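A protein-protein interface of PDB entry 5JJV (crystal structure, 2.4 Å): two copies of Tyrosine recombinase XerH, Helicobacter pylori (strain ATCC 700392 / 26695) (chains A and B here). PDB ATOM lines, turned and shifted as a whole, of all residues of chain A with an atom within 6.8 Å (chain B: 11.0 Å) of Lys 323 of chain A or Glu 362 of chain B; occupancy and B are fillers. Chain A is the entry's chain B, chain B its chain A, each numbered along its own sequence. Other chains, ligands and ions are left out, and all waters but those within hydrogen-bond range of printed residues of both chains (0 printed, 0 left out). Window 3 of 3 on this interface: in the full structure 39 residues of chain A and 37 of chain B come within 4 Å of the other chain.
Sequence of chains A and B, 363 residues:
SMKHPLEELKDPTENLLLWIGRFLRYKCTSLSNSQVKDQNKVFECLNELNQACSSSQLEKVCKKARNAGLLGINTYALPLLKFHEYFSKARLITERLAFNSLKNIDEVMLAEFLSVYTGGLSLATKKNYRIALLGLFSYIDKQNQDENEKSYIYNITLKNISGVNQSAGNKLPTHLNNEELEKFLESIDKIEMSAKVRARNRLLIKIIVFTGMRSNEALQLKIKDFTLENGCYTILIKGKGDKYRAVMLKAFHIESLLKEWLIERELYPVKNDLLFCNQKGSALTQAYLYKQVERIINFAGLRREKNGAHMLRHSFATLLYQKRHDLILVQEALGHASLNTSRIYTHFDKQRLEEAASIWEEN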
ATOM      1  N   ASN A 178       0.134   0.321 -19.485  1.00  0.00           N
ATOM      2  CA  ASN A 178      -0.874  -0.663 -19.861  1.00  0.00           C
ATOM      3  C   ASN A 178      -1.229  -1.592 -18.703  1.00  0.00           C
ATOM      4  O   ASN A 178      -2.405  -1.822 -18.420  1.00  0.00           O
ATOM      5  CB  ASN A 178      -0.393  -1.481 -21.062  1.00  0.00           C
ATOM      6  CG  ASN A 178      -1.541  -2.042 -21.883  1.00  0.00           C
ATOM      7  OD1 ASN A 178      -2.661  -2.186 -21.391  1.00  0.00           O
ATOM      8  ND2 ASN A 178      -1.267  -2.358 -23.144  1.00  0.00           N
ATOM      9  N   THR A 318      -1.818   8.004 -23.772  1.00  0.00           N
ATOM     10  CA  THR A 318      -0.593   7.222 -23.886  1.00  0.00           C
ATOM     11  C   THR A 318      -0.870   5.833 -24.450  1.00  0.00           C
ATOM     12  O   THR A 318      -0.161   5.365 -25.340  1.00  0.00           O
ATOM     13  CB  THR A 318       0.111   7.088 -22.527  1.00  0.00           C
ATOM     14  OG1 THR A 318       0.535   8.384 -22.085  1.00  0.00           O
ATOM     15  CG2 THR A 318       1.325   6.175 -22.637  1.00  0.00           C
ATOM     16  N   LEU A 319      -1.907   5.184 -23.933  1.00  0.00           N
ATOM     17  CA  LEU A 319      -2.309   3.870 -24.424  1.00  0.00           C
ATOM     18  C   LEU A 319      -2.810   3.949 -25.860  1.00  0.00           C
ATOM     19  O   LEU A 319      -2.501   3.088 -26.684  1.00  0.00           O
ATOM     20  CB  LEU A 319      -3.397   3.271 -23.534  1.00  0.00           C
ATOM     21  CG  LEU A 319      -3.948   1.926 -24.012  1.00  0.00           C
ATOM     22  CD1 LEU A 319      -2.887   0.840 -23.906  1.00  0.00           C
ATOM     23  CD2 LEU A 319      -5.193   1.542 -23.236  1.00  0.00           C
ATOM     24  N   LEU A 320      -3.587   4.990 -26.149  1.00  0.00           N
ATOM     25  CA  LEU A 320      -4.172   5.179 -27.472  1.00  0.00           C
ATOM     26  C   LEU A 320      -3.102   5.282 -28.554  1.00  0.00           C
ATOM     27  O   LEU A 320      -3.221   4.660 -29.610  1.00  0.00           O
ATOM     28  CB  LEU A 320      -5.060   6.425 -27.489  1.00  0.00           C
ATOM     29  CG  LEU A 320      -5.666   6.835 -28.833  1.00  0.00           C
ATOM     30  CD1 LEU A 320      -6.404   5.672 -29.483  1.00  0.00           C
ATOM     31  CD2 LEU A 320      -6.596   8.028 -28.651  1.00  0.00           C
ATOM     32  N   TYR A 321      -2.058   6.063 -28.291  1.00  0.00           N
ATOM     33  CA  TYR A 321      -0.968   6.190 -29.250  1.00  0.00           C
ATOM     34  C   TYR A 321      -0.133   4.917 -29.293  1.00  0.00           C
ATOM     35  O   TYR A 321       0.386   4.541 -30.342  1.00  0.00           O
ATOM     36  CB  TYR A 321      -0.070   7.384 -28.923  1.00  0.00           C
ATOM     37  CG  TYR A 321       1.033   7.581 -29.941  1.00  0.00           C
ATOM     38  CD1 TYR A 321       0.814   8.328 -31.092  1.00  0.00           C
ATOM     39  CD2 TYR A 321       2.286   7.004 -29.766  1.00  0.00           C
ATOM     40  CE1 TYR A 321       1.810   8.504 -32.031  1.00  0.00           C
ATOM     41  CE2 TYR A 321       3.287   7.173 -30.703  1.00  0.00           C
ATOM     42  CZ  TYR A 321       3.044   7.924 -31.834  1.00  0.00           C
ATOM     43  OH  TYR A 321       4.035   8.101 -32.771  1.00  0.00           O
ATOM     44  N   GLN A 322       0.004   4.264 -28.144  1.00  0.00           N
ATOM     45  CA  GLN A 322       0.764   3.023 -28.058  1.00  0.00           C
ATOM     46  C   GLN A 322       0.166   1.952 -28.965  1.00  0.00           C
ATOM     47  O   GLN A 322       0.887   1.137 -29.542  1.00  0.00           O
ATOM     48  CB  GLN A 322       0.815   2.525 -26.612  1.00  0.00           C
ATOM     49  CG  GLN A 322       1.568   1.221 -26.428  1.00  0.00           C
ATOM     50  CD  GLN A 322       1.537   0.729 -24.994  1.00  0.00           C
ATOM     51  OE1 GLN A 322       1.565   1.522 -24.053  1.00  0.00           O
ATOM     52  NE2 GLN A 322       1.469  -0.588 -24.822  1.00  0.00           N
ATOM     53  N   LYS A 323      -1.156   1.971 -29.102  1.00  0.00           N
ATOM     54  CA  LYS A 323      -1.855   0.961 -29.886  1.00  0.00           C
ATOM     55  C   LYS A 323      -2.063   1.371 -31.343  1.00  0.00           C
ATOM     56  O   LYS A 323      -2.248   0.517 -32.208  1.00  0.00           O
ATOM     57  CB  LYS A 323      -3.210   0.643 -29.245  1.00  0.00           C
ATOM     58  CG  LYS A 323      -3.117   0.067 -27.841  1.00  0.00           C
ATOM     59  CD  LYS A 323      -2.364  -1.253 -27.833  1.00  0.00           C
ATOM     60  CE  LYS A 323      -2.342  -1.873 -26.443  1.00  0.00           C
ATOM     61  NZ  LYS A 323      -1.659  -3.197 -26.431  1.00  0.00           N
ATOM     62  N   ARG A 324      -2.031   2.672 -31.620  1.00  0.00           N
ATOM     63  CA  ARG A 324      -2.386   3.156 -32.952  1.00  0.00           C
ATOM     64  C   ARG A 324      -1.288   3.964 -33.648  1.00  0.00           C
ATOM     65  O   ARG A 324      -1.315   4.111 -34.870  1.00  0.00           O
ATOM     66  CB  ARG A 324      -3.660   3.999 -32.873  1.00  0.00           C
ATOM     67  CG  ARG A 324      -4.888   3.224 -32.421  1.00  0.00           C
ATOM     68  CD  ARG A 324      -5.260   2.152 -33.428  1.00  0.00           C
ATOM     69  NE  ARG A 324      -6.455   1.416 -33.025  1.00  0.00           N
ATOM     70  CZ  ARG A 324      -6.436   0.232 -32.422  1.00  0.00           C
ATOM     71  NH1 ARG A 324      -5.280  -0.358 -32.154  1.00  0.00           N
ATOM     72  NH2 ARG A 324      -7.574  -0.365 -32.089  1.00  0.00           N
ATOM     73  N   HIS A 325      -0.338   4.486 -32.874  1.00  0.00           N
ATOM     74  CA  HIS A 325       0.732   5.337 -33.402  1.00  0.00           C
ATOM     75  C   HIS A 325       0.186   6.501 -34.227  1.00  0.00           C
ATOM     76  O   HIS A 325       0.788   6.902 -35.223  1.00  0.00           O
ATOM     77  CB  HIS A 325       1.713   4.518 -34.250  1.00  0.00           C
ATOM     78  CG  HIS A 325       2.572   3.585 -33.454  1.00  0.00           C
ATOM     79  ND1 HIS A 325       3.444   2.694 -34.040  1.00  0.00           N
ATOM     80  CD2 HIS A 325       2.694   3.407 -32.116  1.00  0.00           C
ATOM     81  CE1 HIS A 325       4.067   2.006 -33.099  1.00  0.00           C
ATOM     82  NE2 HIS A 325       3.629   2.419 -31.924  1.00  0.00           N
ATOM     83  N   ASP A 326      -0.955   7.040 -33.804  1.00  0.00           N
ATOM     84  CA  ASP A 326      -1.622   8.112 -34.537  1.00  0.00           C
ATOM     85  C   ASP A 326      -1.919   9.291 -33.614  1.00  0.00           C
ATOM     86  O   ASP A 326      -2.896   9.273 -32.865  1.00  0.00           O
ATOM     87  CB  ASP A 326      -2.915   7.595 -35.174  1.00  0.00           C
ATOM     88  CG  ASP A 326      -3.490   8.554 -36.200  1.00  0.00           C
ATOM     89  OD1 ASP A 326      -3.048   9.721 -36.261  1.00  0.00           O
ATOM     90  OD2 ASP A 326      -4.399   8.137 -36.948  1.00  0.00           O
ATOM     91  N   LEU B 353     -14.095   6.733 -34.895  1.00  0.00           N
ATOM     92  CA  LEU B 353     -14.292   6.631 -33.454  1.00  0.00           C
ATOM     93  C   LEU B 353     -13.976   5.226 -32.951  1.00  0.00           C
ATOM     94  O   LEU B 353     -13.458   5.051 -31.847  1.00  0.00           O
ATOM     95  CB  LEU B 353     -15.727   7.012 -33.084  1.00  0.00           C
ATOM     96  CG  LEU B 353     -16.120   8.478 -33.274  1.00  0.00           C
ATOM     97  CD1 LEU B 353     -17.621   8.666 -33.107  1.00  0.00           C
ATOM     98  CD2 LEU B 353     -15.360   9.357 -32.295  1.00  0.00           C
ATOM     99  N   GLU B 354     -14.294   4.232 -33.774  1.00  0.00           N
ATOM    100  CA  GLU B 354     -14.038   2.832 -33.455  1.00  0.00           C
ATOM    101  C   GLU B 354     -12.555   2.574 -33.195  1.00  0.00           C
ATOM    102  O   GLU B 354     -12.201   1.808 -32.300  1.00  0.00           O
ATOM    103  CB  GLU B 354     -14.535   1.934 -34.592  1.00  0.00           C
ATOM    104  CG  GLU B 354     -14.242   0.453 -34.408  1.00  0.00           C
ATOM    105  CD  GLU B 354     -15.265  -0.241 -33.533  1.00  0.00           C
ATOM    106  OE1 GLU B 354     -16.333   0.356 -33.281  1.00  0.00           O
ATOM    107  OE2 GLU B 354     -15.003  -1.383 -33.101  1.00  0.00           O
ATOM    108  N   GLU B 355     -11.698   3.224 -33.979  1.00  0.00           N
ATOM    109  CA  GLU B 355     -10.250   3.039 -33.871  1.00  0.00           C
ATOM    110  C   GLU B 355      -9.729   3.370 -32.478  1.00  0.00           C
ATOM    111  O   GLU B 355      -8.780   2.751 -31.999  1.00  0.00           O
ATOM    112  CB  GLU B 355      -9.518   3.901 -34.902  1.00  0.00           C
ATOM    113  CG  GLU B 355      -9.876   3.601 -36.343  1.00  0.00           C
ATOM    114  CD  GLU B 355      -9.043   4.402 -37.325  1.00  0.00           C
ATOM    115  OE1 GLU B 355      -7.872   4.696 -37.007  1.00  0.00           O
ATOM    116  OE2 GLU B 355      -9.563   4.741 -38.411  1.00  0.00           O
ATOM    117  N   ALA B 356     -10.351   4.353 -31.834  1.00  0.00           N
ATOM    118  CA  ALA B 356      -9.922   4.783 -30.510  1.00  0.00           C
ATOM    119  C   ALA B 356     -10.543   3.921 -29.418  1.00  0.00           C
ATOM    120  O   ALA B 356      -9.864   3.505 -28.480  1.00  0.00           O
ATOM    121  CB  ALA B 356     -10.271   6.247 -30.292  1.00  0.00           C
ATOM    122  N   ALA B 357     -11.837   3.650 -29.549  1.00  0.00           N
ATOM    123  CA  ALA B 357     -12.580   2.924 -28.526  1.00  0.00           C
ATOM    124  C   ALA B 357     -12.164   1.458 -28.414  1.00  0.00           C
ATOM    125  O   ALA B 357     -12.389   0.824 -27.383  1.00  0.00           O
ATOM    126  CB  ALA B 357     -14.073   3.017 -28.801  1.00  0.00           C
ATOM    127  N   SER B 358     -11.558   0.926 -29.470  1.00  0.00           N
ATOM    128  CA  SER B 358     -11.248  -0.500 -29.528  1.00  0.00           C
ATOM    129  C   SER B 358      -9.851  -0.842 -29.015  1.00  0.00           C
ATOM    130  O   SER B 358      -9.399  -1.979 -29.158  1.00  0.00           O
ATOM    131  CB  SER B 358     -11.402  -1.013 -30.961  1.00  0.00           C
ATOM    132  OG  SER B 358     -10.459  -0.400 -31.823  1.00  0.00           O
ATOM    133  N   ILE B 359      -9.168   0.130 -28.416  1.00  0.00           N
ATOM    134  CA  ILE B 359      -7.823  -0.109 -27.898  1.00  0.00           C
ATOM    135  C   ILE B 359      -7.858  -0.988 -26.652  1.00  0.00           C
ATOM    136  O   ILE B 359      -6.852  -1.589 -26.278  1.00  0.00           O
ATOM    137  CB  ILE B 359      -7.088   1.206 -27.560  1.00  0.00           C
ATOM    138  CG1 ILE B 359      -7.808   1.952 -26.436  1.00  0.00           C
ATOM    139  CG2 ILE B 359      -6.953   2.078 -28.801  1.00  0.00           C
ATOM    140  CD1 ILE B 359      -7.133   3.242 -26.027  1.00  0.00           C
ATOM    141  N   TRP B 360      -9.025  -1.065 -26.021  1.00  0.00           N
ATOM    142  CA  TRP B 360      -9.189  -1.847 -24.802  1.00  0.00           C
ATOM    143  C   TRP B 360      -9.438  -3.324 -25.099  1.00  0.00           C
ATOM    144  O   TRP B 360      -9.346  -4.169 -24.208  1.00  0.00           O
ATOM    145  CB  TRP B 360     -10.336  -1.278 -23.966  1.00  0.00           C
ATOM    146  CG  TRP B 360     -10.184   0.179 -23.684  1.00  0.00           C
ATOM    147  CD1 TRP B 360     -10.808   1.209 -24.326  1.00  0.00           C
ATOM    148  CD2 TRP B 360      -9.342   0.777 -22.691  1.00  0.00           C
ATOM    149  NE1 TRP B 360     -10.412   2.411 -23.790  1.00  0.00           N
ATOM    150  CE2 TRP B 360      -9.511   2.173 -22.785  1.00  0.00           C
ATOM    151  CE3 TRP B 360      -8.465   0.267 -21.730  1.00  0.00           C
ATOM    152  CZ2 TRP B 360      -8.837   3.064 -21.954  1.00  0.00           C
ATOM    153  CZ3 TRP B 360      -7.796   1.153 -20.906  1.00  0.00           C
ATOM    154  CH2 TRP B 360      -7.984   2.535 -21.024  1.00  0.00           C
ATOM    155  N   GLU B 361      -9.748  -3.628 -26.356  1.00  0.00           N
ATOM    156  CA  GLU B 361     -10.021  -5.000 -26.775  1.00  0.00           C
ATOM    157  C   GLU B 361      -8.743  -5.744 -27.144  1.00  0.00           C
ATOM    158  O   GLU B 361      -8.795  -6.848 -27.683  1.00  0.00           O
ATOM    159  CB  GLU B 361     -10.985  -5.007 -27.963  1.00  0.00           C
ATOM    160  CG  GLU B 361     -12.329  -4.363 -27.674  1.00  0.00           C
ATOM    161  CD  GLU B 361     -13.026  -3.873 -28.929  1.00  0.00           C
ATOM    162  OE1 GLU B 361     -12.602  -4.262 -30.039  1.00  0.00           O
ATOM    163  OE2 GLU B 361     -13.992  -3.092 -28.806  1.00  0.00           O
ATOM    164  N   GLU B 362      -7.597  -5.137 -26.852  1.00  0.00           N
ATOM    165  CA  GLU B 362      -6.310  -5.714 -27.223  1.00  0.00           C
ATOM    166  C   GLU B 362      -5.412  -5.921 -26.009  1.00  0.00           C
ATOM    167  O   GLU B 362      -4.532  -6.782 -26.016  1.00  0.00           O
ATOM    168  CB  GLU B 362      -5.609  -4.822 -28.248  1.00  0.00           C
ATOM    169  CG  GLU B 362      -6.468  -4.481 -29.455  1.00  0.00           C
ATOM    170  CD  GLU B 362      -5.789  -3.512 -30.402  1.00  0.00           C
ATOM    171  OE1 GLU B 362      -6.469  -2.997 -31.313  1.00  0.00           O
ATOM    172  OE2 GLU B 362      -4.575  -3.269 -30.235  1.00  0.00           O
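OE1 of Glu 362 of chain B lies within salt-bridge range of NH2 of Arg 324 of chain A, at 3.0 Å. The guanidinium group (NH2) of Arg 324 of chain A is in hydrogen-bond range of the side-chain hydroxyl (OG) of Ser 358 of chain B, 2.9 Å away. The backbone carbonyl oxygen of Glu 355 of chain B is in hydrogen-bond range of the guanidinium group of Arg 324 of chain A (2.9 Å).
O of Glu 354 of chain B is in hydrogen-bond range of OG of Ser 358 of chain B (2.9 Å). NZ of Lys 323 of chain A sits close to ND2 of Asn 178 of chain A.
Among the printed residues, merely in contact across the chains: Leu 319 of chain A with Trp 360 of chain B, Leu 320 of chain A with Ile 359 of chain B, Leu 320 of chain A with Ala 356 of chain B, Leu 319 of chain A with Ile 359 of chain B and Lys 323 of chain A with Glu 362 of chain B.
Lys 323 of chain A touches just one residue of chain B: Glu 362. Of chain A, only Lys 323 and Arg 324 come within 4 Å of Glu 362 of chain B. Of chain B, only Ile 359 and Trp 360 come within 4 Å of Leu 319 of chain A. No residue of chain B comes within 4 Å of Gln 322 of chain A. Arg 324 of chain A touches just these residues of chain B: Glu 355, Ser 358 and Glu 362. Of the printed residues of chain A, Glu 355 of chain B touches Arg 324. Of the printed residues of chain A, Ala 356 of chain B touches Leu 320 (3.8 Å). Of the printed residues of chain A, Ser 358 of chain B touches Arg 324. Printed residues of chain A within 4 Å of Ile 359 of chain B: Leu 319 (3.8 Å) and Leu 320 (3.7 Å). Asp 326 of chain A touches none of the printed residues of chain B.
Along chain B the printed residues that touch a printed residue of chain A span positions 355 to 362. Among the printed residues, 8 pairs touch across the chains. Among the printed residues, Asp or Glu carboxylates within 4 Å of a Lys or Arg side-chain nitrogen of the other chain: Arg 324 of chain A with Glu 362 of chain B (3.0 Å).
No position is printed for both chains. Of the 8 pairs that touch across the chains among the printed residues, none has its exchanged pair printed and touching as well.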
